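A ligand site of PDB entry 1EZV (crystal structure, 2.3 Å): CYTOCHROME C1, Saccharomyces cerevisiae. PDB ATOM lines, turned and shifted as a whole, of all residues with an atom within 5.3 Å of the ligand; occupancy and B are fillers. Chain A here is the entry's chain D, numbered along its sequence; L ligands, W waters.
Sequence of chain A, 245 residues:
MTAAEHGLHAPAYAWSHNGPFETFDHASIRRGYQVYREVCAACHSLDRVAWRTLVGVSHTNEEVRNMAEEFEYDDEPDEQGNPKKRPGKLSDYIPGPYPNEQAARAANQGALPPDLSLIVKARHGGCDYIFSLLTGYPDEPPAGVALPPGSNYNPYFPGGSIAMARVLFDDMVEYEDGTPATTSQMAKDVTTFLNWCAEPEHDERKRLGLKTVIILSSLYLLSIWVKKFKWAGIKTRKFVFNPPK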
ATOM      1  N   VAL A  35       5.710 -26.002  35.763  1.00  0.00           N
ATOM      2  CA  VAL A  35       5.228 -26.338  34.420  1.00  0.00           C
ATOM      3  C   VAL A  35       4.262 -25.264  33.934  1.00  0.00           C
ATOM      4  O   VAL A  35       4.331 -24.848  32.779  1.00  0.00           O
ATOM      5  CB  VAL A  35       4.525 -27.707  34.410  1.00  0.00           C
ATOM      6  CG1 VAL A  35       3.957 -27.999  33.027  1.00  0.00           C
ATOM      7  CG2 VAL A  35       5.503 -28.796  34.828  1.00  0.00           C
ATOM      8  N   VAL A  39       5.687 -23.239  30.764  1.00  0.00           N
ATOM      9  CA  VAL A  39       4.998 -23.619  29.525  1.00  0.00           C
ATOM     10  C   VAL A  39       3.669 -22.860  29.339  1.00  0.00           C
ATOM     11  O   VAL A  39       3.576 -21.959  28.499  1.00  0.00           O
ATOM     12  CB  VAL A  39       4.743 -25.137  29.483  1.00  0.00           C
ATOM     13  CG1 VAL A  39       4.338 -25.564  28.078  1.00  0.00           C
ATOM     14  CG2 VAL A  39       5.983 -25.901  29.933  1.00  0.00           C
ATOM     15  N   CYS A  40       2.707 -23.140  30.224  1.00  0.00           N
ATOM     16  CA  CYS A  40       1.317 -22.719  30.027  1.00  0.00           C
ATOM     17  C   CYS A  40       1.064 -21.214  30.111  1.00  0.00           C
ATOM     18  O   CYS A  40       0.250 -20.681  29.355  1.00  0.00           O
ATOM     19  CB  CYS A  40       0.409 -23.421  31.031  1.00  0.00           C
ATOM     20  SG  CYS A  40       0.801 -25.181  31.282  1.00  0.00           S
ATOM     21  N   ALA A  42       2.319 -18.693  29.068  1.00  0.00           N
ATOM     22  CA  ALA A  42       2.560 -17.892  27.873  1.00  0.00           C
ATOM     23  C   ALA A  42       1.260 -17.614  27.125  1.00  0.00           C
ATOM     24  O   ALA A  42       1.163 -16.634  26.369  1.00  0.00           O
ATOM     25  CB  ALA A  42       3.558 -18.602  26.966  1.00  0.00           C
ATOM     26  N   CYS A  43       0.263 -18.479  27.324  1.00  0.00           N
ATOM     27  CA  CYS A  43      -1.037 -18.318  26.688  1.00  0.00           C
ATOM     28  C   CYS A  43      -2.225 -18.291  27.656  1.00  0.00           C
ATOM     29  O   CYS A  43      -3.307 -17.834  27.288  1.00  0.00           O
ATOM     30  CB  CYS A  43      -1.263 -19.444  25.664  1.00  0.00           C
ATOM     31  SG  CYS A  43       0.133 -19.749  24.550  1.00  0.00           S
ATOM     32  N   HIS A  44      -2.043 -18.839  28.862  1.00  0.00           N
ATOM     33  CA  HIS A  44      -3.135 -19.055  29.808  1.00  0.00           C
ATOM     34  C   HIS A  44      -3.017 -18.178  31.057  1.00  0.00           C
ATOM     35  O   HIS A  44      -2.075 -18.333  31.837  1.00  0.00           O
ATOM     36  CB  HIS A  44      -3.172 -20.524  30.269  1.00  0.00           C
ATOM     37  CG  HIS A  44      -3.765 -21.451  29.257  1.00  0.00           C
ATOM     38  ND1 HIS A  44      -5.050 -21.357  28.769  1.00  0.00           N
ATOM     39  CD2 HIS A  44      -3.231 -22.552  28.660  1.00  0.00           C
ATOM     40  CE1 HIS A  44      -5.242 -22.366  27.911  1.00  0.00           C
ATOM     41  NE2 HIS A  44      -4.158 -23.115  27.803  1.00  0.00           N
ATOM     42  N   ASN A 108      -3.306 -16.238  18.901  1.00  0.00           N
ATOM     43  CA  ASN A 108      -3.660 -17.655  18.839  1.00  0.00           C
ATOM     44  C   ASN A 108      -4.608 -17.987  17.689  1.00  0.00           C
ATOM     45  O   ASN A 108      -5.534 -18.791  17.862  1.00  0.00           O
ATOM     46  CB  ASN A 108      -4.290 -18.103  20.155  1.00  0.00           C
ATOM     47  CG  ASN A 108      -3.324 -18.074  21.300  1.00  0.00           C
ATOM     48  OD1 ASN A 108      -2.601 -19.037  21.525  1.00  0.00           O
ATOM     49  ND2 ASN A 108      -3.257 -16.947  21.998  1.00  0.00           N
ATOM     50  N   ALA A 111      -8.264 -17.824  18.398  1.00  0.00           N
ATOM     51  CA  ALA A 111      -8.801 -18.643  19.468  1.00  0.00           C
ATOM     52  C   ALA A 111      -8.498 -18.053  20.853  1.00  0.00           C
ATOM     53  O   ALA A 111      -7.517 -17.317  21.017  1.00  0.00           O
ATOM     54  CB  ALA A 111      -8.250 -20.049  19.374  1.00  0.00           C
ATOM     55  N   LEU A 112      -9.347 -18.356  21.831  1.00  0.00           N
ATOM     56  CA  LEU A 112      -9.197 -17.795  23.162  1.00  0.00           C
ATOM     57  C   LEU A 112      -8.839 -18.869  24.179  1.00  0.00           C
ATOM     58  O   LEU A 112      -9.653 -19.741  24.508  1.00  0.00           O
ATOM     59  CB  LEU A 112     -10.498 -17.097  23.562  1.00  0.00           C
ATOM     60  CG  LEU A 112     -10.507 -16.279  24.850  1.00  0.00           C
ATOM     61  CD1 LEU A 112      -9.488 -15.145  24.785  1.00  0.00           C
ATOM     62  CD2 LEU A 112     -11.911 -15.728  25.058  1.00  0.00           C
ATOM     63  N   PRO A 113      -7.576 -18.869  24.642  1.00  0.00           N
ATOM     64  CA  PRO A 113      -7.164 -19.814  25.691  1.00  0.00           C
ATOM     65  C   PRO A 113      -7.873 -19.496  27.005  1.00  0.00           C
ATOM     66  O   PRO A 113      -7.723 -18.396  27.539  1.00  0.00           O
ATOM     67  CB  PRO A 113      -5.650 -19.590  25.800  1.00  0.00           C
ATOM     68  CG  PRO A 113      -5.286 -18.730  24.616  1.00  0.00           C
ATOM     69  CD  PRO A 113      -6.495 -17.937  24.288  1.00  0.00           C
ATOM     70  N   PRO A 114      -8.722 -20.421  27.492  1.00  0.00           N
ATOM     71  CA  PRO A 114      -9.458 -20.161  28.729  1.00  0.00           C
ATOM     72  C   PRO A 114      -8.532 -19.973  29.921  1.00  0.00           C
ATOM     73  O   PRO A 114      -7.397 -20.461  29.929  1.00  0.00           O
ATOM     74  CB  PRO A 114     -10.328 -21.393  28.888  1.00  0.00           C
ATOM     75  CG  PRO A 114      -9.542 -22.467  28.241  1.00  0.00           C
ATOM     76  CD  PRO A 114      -8.937 -21.802  27.033  1.00  0.00           C
ATOM     77  N   LEU A 116      -7.417 -20.856  33.607  1.00  0.00           N
ATOM     78  CA  LEU A 116      -7.290 -22.213  34.098  1.00  0.00           C
ATOM     79  C   LEU A 116      -7.601 -22.356  35.590  1.00  0.00           C
ATOM     80  O   LEU A 116      -7.494 -23.455  36.149  1.00  0.00           O
ATOM     81  CB  LEU A 116      -5.896 -22.762  33.801  1.00  0.00           C
ATOM     82  CG  LEU A 116      -5.535 -23.003  32.334  1.00  0.00           C
ATOM     83  CD1 LEU A 116      -4.179 -23.709  32.235  1.00  0.00           C
ATOM     84  CD2 LEU A 116      -6.610 -23.839  31.644  1.00  0.00           C
ATOM     85  N   ILE A 119     -10.582 -24.690  35.583  1.00  0.00           N
ATOM     86  CA  ILE A 119     -10.707 -25.587  34.424  1.00  0.00           C
ATOM     87  C   ILE A 119     -10.945 -27.052  34.803  1.00  0.00           C
ATOM     88  O   ILE A 119     -11.713 -27.738  34.132  1.00  0.00           O
ATOM     89  CB  ILE A 119      -9.476 -25.450  33.459  1.00  0.00           C
ATOM     90  CG1 ILE A 119      -9.931 -25.727  32.024  1.00  0.00           C
ATOM     91  CG2 ILE A 119      -8.331 -26.395  33.857  1.00  0.00           C
ATOM     92  CD1 ILE A 119     -10.805 -24.617  31.450  1.00  0.00           C
ATOM     93  N   ARG A 123     -15.043 -28.923  33.511  1.00  0.00           N
ATOM     94  CA  ARG A 123     -15.040 -29.938  32.462  1.00  0.00           C
ATOM     95  C   ARG A 123     -15.424 -31.287  33.044  1.00  0.00           C
ATOM     96  O   ARG A 123     -14.959 -31.644  34.127  1.00  0.00           O
ATOM     97  CB  ARG A 123     -13.644 -30.042  31.802  1.00  0.00           C
ATOM     98  CG  ARG A 123     -13.169 -28.803  31.052  1.00  0.00           C
ATOM     99  CD  ARG A 123     -13.975 -28.533  29.791  1.00  0.00           C
ATOM    100  NE  ARG A 123     -13.417 -27.432  29.013  1.00  0.00           N
ATOM    101  CZ  ARG A 123     -13.601 -26.131  29.272  1.00  0.00           C
ATOM    102  NH1 ARG A 123     -12.950 -25.226  28.557  1.00  0.00           N
ATOM    103  NH2 ARG A 123     -14.474 -25.748  30.200  1.00  0.00           N
ATOM    104  N   TYR A 129      -9.584 -35.893  32.449  1.00  0.00           N
ATOM    105  CA  TYR A 129      -9.757 -35.250  31.150  1.00  0.00           C
ATOM    106  C   TYR A 129      -8.541 -34.404  30.804  1.00  0.00           C
ATOM    107  O   TYR A 129      -7.945 -34.586  29.756  1.00  0.00           O
ATOM    108  CB  TYR A 129     -11.031 -34.401  31.142  1.00  0.00           C
ATOM    109  CG  TYR A 129     -11.161 -33.525  29.929  1.00  0.00           C
ATOM    110  CD1 TYR A 129     -11.326 -34.081  28.656  1.00  0.00           C
ATOM    111  CD2 TYR A 129     -11.000 -32.144  30.026  1.00  0.00           C
ATOM    112  CE1 TYR A 129     -11.330 -33.286  27.517  1.00  0.00           C
ATOM    113  CE2 TYR A 129     -11.020 -31.343  28.886  1.00  0.00           C
ATOM    114  CZ  TYR A 129     -11.170 -31.921  27.639  1.00  0.00           C
ATOM    115  OH  TYR A 129     -11.173 -31.138  26.511  1.00  0.00           O
ATOM    116  N   ILE A 130      -8.175 -33.486  31.704  1.00  0.00           N
ATOM    117  CA  ILE A 130      -7.078 -32.551  31.471  1.00  0.00           C
ATOM    118  C   ILE A 130      -5.780 -33.297  31.147  1.00  0.00           C
ATOM    119  O   ILE A 130      -5.068 -32.958  30.201  1.00  0.00           O
ATOM    120  CB  ILE A 130      -6.816 -31.667  32.707  1.00  0.00           C
ATOM    121  CG1 ILE A 130      -8.123 -31.008  33.185  1.00  0.00           C
ATOM    122  CG2 ILE A 130      -5.760 -30.623  32.391  1.00  0.00           C
ATOM    123  CD1 ILE A 130      -8.650 -29.923  32.270  1.00  0.00           C
ATOM    124  N   LEU A 133      -6.047 -35.106  27.719  1.00  0.00           N
ATOM    125  CA  LEU A 133      -5.942 -34.144  26.623  1.00  0.00           C
ATOM    126  C   LEU A 133      -4.474 -33.816  26.337  1.00  0.00           C
ATOM    127  O   LEU A 133      -4.039 -33.881  25.190  1.00  0.00           O
ATOM    128  CB  LEU A 133      -6.705 -32.856  26.972  1.00  0.00           C
ATOM    129  CG  LEU A 133      -6.721 -31.782  25.869  1.00  0.00           C
ATOM    130  CD1 LEU A 133      -7.753 -32.127  24.813  1.00  0.00           C
ATOM    131  CD2 LEU A 133      -7.002 -30.407  26.469  1.00  0.00           C
ATOM    132  N   LEU A 134      -3.713 -33.549  27.398  1.00  0.00           N
ATOM    133  CA  LEU A 134      -2.338 -33.067  27.268  1.00  0.00           C
ATOM    134  C   LEU A 134      -1.380 -34.144  26.758  1.00  0.00           C
ATOM    135  O   LEU A 134      -0.357 -33.825  26.158  1.00  0.00           O
ATOM    136  CB  LEU A 134      -1.823 -32.528  28.607  1.00  0.00           C
ATOM    137  CG  LEU A 134      -2.398 -31.210  29.118  1.00  0.00           C
ATOM    138  CD1 LEU A 134      -2.021 -31.028  30.583  1.00  0.00           C
ATOM    139  CD2 LEU A 134      -1.896 -30.051  28.279  1.00  0.00           C
ATOM    140  N   PHE A 157     -10.843 -34.284  22.873  1.00  0.00           N
ATOM    141  CA  PHE A 157     -11.604 -33.051  22.679  1.00  0.00           C
ATOM    142  C   PHE A 157     -12.837 -33.349  21.816  1.00  0.00           C
ATOM    143  O   PHE A 157     -12.752 -34.094  20.838  1.00  0.00           O
ATOM    144  CB  PHE A 157     -10.717 -32.022  21.994  1.00  0.00           C
ATOM    145  CG  PHE A 157     -11.267 -30.625  22.027  1.00  0.00           C
ATOM    146  CD1 PHE A 157     -11.380 -29.932  23.231  1.00  0.00           C
ATOM    147  CD2 PHE A 157     -11.653 -29.988  20.848  1.00  0.00           C
ATOM    148  CE1 PHE A 157     -11.871 -28.611  23.263  1.00  0.00           C
ATOM    149  CE2 PHE A 157     -12.152 -28.678  20.861  1.00  0.00           C
ATOM    150  CZ  PHE A 157     -12.260 -27.984  22.073  1.00  0.00           C
ATOM    151  N   SER A 161     -11.111 -31.582  16.834  1.00  0.00           N
ATOM    152  CA  SER A 161     -10.330 -30.476  16.291  1.00  0.00           C
ATOM    153  C   SER A 161     -10.124 -29.357  17.318  1.00  0.00           C
ATOM    154  O   SER A 161     -11.025 -28.555  17.578  1.00  0.00           O
ATOM    155  CB  SER A 161     -11.019 -29.954  15.029  1.00  0.00           C
ATOM    156  OG  SER A 161     -10.459 -28.718  14.609  1.00  0.00           O
ATOM    157  N   ILE A 162      -8.918 -29.287  17.878  1.00  0.00           N
ATOM    158  CA  ILE A 162      -8.615 -28.338  18.953  1.00  0.00           C
ATOM    159  C   ILE A 162      -7.561 -27.318  18.542  1.00  0.00           C
ATOM    160  O   ILE A 162      -6.589 -27.662  17.860  1.00  0.00           O
ATOM    161  CB  ILE A 162      -8.141 -29.091  20.220  1.00  0.00           C
ATOM    162  CG1 ILE A 162      -8.013 -28.112  21.399  1.00  0.00           C
ATOM    163  CG2 ILE A 162      -6.827 -29.817  19.933  1.00  0.00           C
ATOM    164  CD1 ILE A 162      -7.715 -28.775  22.735  1.00  0.00           C
ATOM    165  N   ALA A 163      -7.711 -26.089  19.010  1.00  0.00           N
ATOM    166  CA  ALA A 163      -6.882 -24.965  18.567  1.00  0.00           C
ATOM    167  C   ALA A 163      -5.581 -24.823  19.352  1.00  0.00           C
ATOM    168  O   ALA A 163      -4.791 -23.916  19.086  1.00  0.00           O
ATOM    169  CB  ALA A 163      -7.677 -23.671  18.611  1.00  0.00           C
ATOM    170  N   MET A 164      -5.384 -25.675  20.338  1.00  0.00           N
ATOM    171  CA  MET A 164      -4.115 -25.746  21.065  1.00  0.00           C
ATOM    172  C   MET A 164      -3.309 -26.918  20.516  1.00  0.00           C
ATOM    173  O   MET A 164      -3.801 -28.041  20.466  1.00  0.00           O
ATOM    174  CB  MET A 164      -4.362 -25.946  22.575  1.00  0.00           C
ATOM    175  CG  MET A 164      -3.110 -26.170  23.402  1.00  0.00           C
ATOM    176  SD  MET A 164      -3.392 -26.199  25.184  1.00  0.00           S
ATOM    177  CE  MET A 164      -4.109 -27.830  25.395  1.00  0.00           C
ATOM    178  N   VAL A 167       1.994 -29.134  23.526  1.00  0.00           N
ATOM    179  CA  VAL A 167       3.029 -28.236  24.047  1.00  0.00           C
ATOM    180  C   VAL A 167       3.979 -28.911  25.041  1.00  0.00           C
ATOM    181  O   VAL A 167       4.995 -28.333  25.415  1.00  0.00           O
ATOM    182  CB  VAL A 167       2.432 -26.980  24.731  1.00  0.00           C
ATOM    183  CG1 VAL A 167       1.600 -26.193  23.739  1.00  0.00           C
ATOM    184  CG2 VAL A 167       1.593 -27.379  25.945  1.00  0.00           C
ATOM    185  N   LEU A 168       3.627 -30.105  25.490  1.00  0.00           N
ATOM    186  CA  LEU A 168       4.481 -30.847  26.393  1.00  0.00           C
ATOM    187  C   LEU A 168       5.358 -31.825  25.622  1.00  0.00           C
ATOM    188  O   LEU A 168       4.846 -32.629  24.830  1.00  0.00           O
ATOM    189  CB  LEU A 168       3.651 -31.615  27.430  1.00  0.00           C
ATOM    190  CG  LEU A 168       2.857 -30.787  28.449  1.00  0.00           C
ATOM    191  CD1 LEU A 168       2.205 -31.718  29.467  1.00  0.00           C
ATOM    192  CD2 LEU A 168       3.784 -29.796  29.138  1.00  0.00           C
ATOM    193  N   VAL A 190       1.031 -30.527  36.450  1.00  0.00           N
ATOM    194  CA  VAL A 190       0.230 -29.305  36.246  1.00  0.00           C
ATOM    195  C   VAL A 190      -1.207 -29.598  36.619  1.00  0.00           C
ATOM    196  O   VAL A 190      -1.915 -28.751  37.134  1.00  0.00           O
ATOM    197  CB  VAL A 190       0.163 -28.799  34.783  1.00  0.00           C
ATOM    198  CG1 VAL A 190       0.971 -27.548  34.641  1.00  0.00           C
ATOM    199  CG2 VAL A 190       0.550 -29.855  33.814  1.00  0.00           C
ATOM    200  N   LEU A 194      -3.504 -27.656  38.984  1.00  0.00           N
ATOM    201  CA  LEU A 194      -4.711 -26.976  38.526  1.00  0.00           C
ATOM    202  C   LEU A 194      -5.945 -27.423  39.320  1.00  0.00           C
ATOM    203  O   LEU A 194      -6.807 -26.607  39.626  1.00  0.00           O
ATOM    204  CB  LEU A 194      -4.903 -27.197  37.021  1.00  0.00           C
ATOM    205  CG  LEU A 194      -3.874 -26.478  36.128  1.00  0.00           C
ATOM    206  CD1 LEU A 194      -4.162 -26.738  34.665  1.00  0.00           C
ATOM    207  CD2 LEU A 194      -3.894 -24.979  36.417  1.00  0.00           C
HETATM  208  C1  LIG L   1      -7.130 -24.617  25.659  1.00  0.00           C
HETATM  209  C2  LIG L   1      -4.481 -26.639  29.124  1.00  0.00           C
HETATM  210  C3  LIG L   1      -0.476 -24.667  27.245  1.00  0.00           C
HETATM  211  C4  LIG L   1      -3.148 -22.439  23.886  1.00  0.00           C
HETATM  212  C5  LIG L   1      -6.768 -25.337  26.785  1.00  0.00           C
HETATM  213  C6  LIG L   1      -7.675 -26.083  27.631  1.00  0.00           C
HETATM  214  C7  LIG L   1      -6.919 -26.693  28.573  1.00  0.00           C
HETATM  215  C8  LIG L   1      -5.552 -26.271  28.353  1.00  0.00           C
HETATM  216  C9  LIG L   1      -7.378 -27.632  29.678  1.00  0.00           C
HETATM  217  C10 LIG L   1      -9.167 -26.179  27.506  1.00  0.00           C
HETATM  218  C11 LIG L   1      -9.583 -27.273  26.548  1.00  0.00           C
HETATM  219  C12 LIG L   1     -11.092 -27.523  26.581  1.00  0.00           C
HETATM  220  O1  LIG L   1     -11.845 -26.618  26.161  1.00  0.00           O
HETATM  221  O2  LIG L   1     -11.507 -28.626  26.998  1.00  0.00           O
HETATM  222  C13 LIG L   1      -3.171 -26.232  28.943  1.00  0.00           C
HETATM  223  C14 LIG L   1      -2.097 -26.508  29.855  1.00  0.00           C
HETATM  224  C15 LIG L   1      -0.961 -26.051  29.283  1.00  0.00           C
HETATM  225  C16 LIG L   1      -1.339 -25.382  28.062  1.00  0.00           C
HETATM  226  C17 LIG L   1      -2.230 -27.197  31.205  1.00  0.00           C
HETATM  227  C18 LIG L   1       0.479 -26.104  29.762  1.00  0.00           C
HETATM  228  C19 LIG L   1       0.901 -27.539  30.045  1.00  0.00           C
HETATM  229  C20 LIG L   1      -0.845 -23.866  26.183  1.00  0.00           C
HETATM  230  C21 LIG L   1       0.028 -22.954  25.475  1.00  0.00           C
HETATM  231  C22 LIG L   1      -0.726 -22.297  24.567  1.00  0.00           C
HETATM  232  C23 LIG L   1      -2.067 -22.828  24.675  1.00  0.00           C
HETATM  233  C24 LIG L   1       1.505 -22.672  25.776  1.00  0.00           C
HETATM  234  C25 LIG L   1      -0.482 -21.149  23.626  1.00  0.00           C
HETATM  235  C26 LIG L   1       0.548 -21.496  22.555  1.00  0.00           C
HETATM  236  C27 LIG L   1      -4.465 -22.848  24.073  1.00  0.00           C
HETATM  237  C28 LIG L   1      -5.554 -22.519  23.194  1.00  0.00           C
HETATM  238  C29 LIG L   1      -6.655 -23.168  23.650  1.00  0.00           C
HETATM  239  C30 LIG L   1      -6.266 -23.861  24.853  1.00  0.00           C
HETATM  240  C31 LIG L   1      -5.415 -21.628  21.968  1.00  0.00           C
HETATM  241  C32 LIG L   1      -8.054 -23.169  23.025  1.00  0.00           C
HETATM  242  C33 LIG L   1      -8.568 -24.507  22.500  1.00  0.00           C
HETATM  243  C34 LIG L   1      -9.781 -24.370  21.577  1.00  0.00           C
HETATM  244  O3  LIG L   1     -10.643 -23.513  21.835  1.00  0.00           O
HETATM  245  O4  LIG L   1      -9.872 -25.129  20.597  1.00  0.00           O
HETATM  246  N1  LIG L   1      -5.479 -25.437  27.258  1.00  0.00           N
HETATM  247  N2  LIG L   1      -2.709 -25.426  27.924  1.00  0.00           N
HETATM  248  N3  LIG L   1      -2.137 -23.677  25.746  1.00  0.00           N
HETATM  249  N4  LIG L   1      -4.913 -23.689  25.071  1.00  0.00           N
HETATM  250 FE1  LIG L   1      -3.815 -24.535  26.488  1.00  0.00          FE
HETATM  251  O   HOH W   1     -10.834 -24.321  24.987  1.00  0.00           O
HETATM  252  O   HOH W   2     -14.226 -29.108  25.923  1.00  0.00           O
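A carbon (C25) of the ligand is bonded to the side-chain sulfur (SG) of Cys 43 (1.8 Å).
SG of Cys 40 is bonded to C18 of the ligand, 1.8 Å away.
FE1 of the ligand is bound by NE2 of His 44 (2.0 Å).
SD of Met 164 is bound to FE1 of the ligand, 2.2 Å away.
The side-chain hydroxyl of Tyr 129 is in hydrogen-bond range of an oxygen (O2) of the ligand, 2.6 Å away.
The backbone NH (N) of Ala 163 sits at hydrogen-bond distance from an oxygen (O4) of the ligand (2.8 Å).
The guanidinium group (NH1) of Arg 123 lies within salt-bridge range of an oxygen (O1) of the ligand (3.0 Å).
Residues that only touch the ligand: Val 39, Phe 157, Ile 162, Pro 114, Val 167, Asn 108, Ile 130, Leu 168, Pro 113, Leu 134, Ile 119 and Leu 194.
Hydrophobic or aromatic side chains within 4 Å of the ligand: His 44, Pro 113, Pro 114, Ile 119, Tyr 129, Ile 130, Leu 134, Phe 157, Ile 162, Ala 163, Met 164, Val 167, Leu 168 and Leu 194.
Of the 27 residues printed, 19 come within 4 Å of the ligand.
Along chain A the residues within 4 Å of the ligand span positions 39 to 194.
The nearest printed residue that does not touch the ligand is Leu 133 (4.1 Å).
The backbone carbonyl oxygen of Val 35 sits at hydrogen-bond distance from the backbone NH of Cys 40 (3.5 Å).
The backbone carbonyl oxygen (O) of Pro 114 is in hydrogen-bond range of a ring nitrogen (ND1) of His 44.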
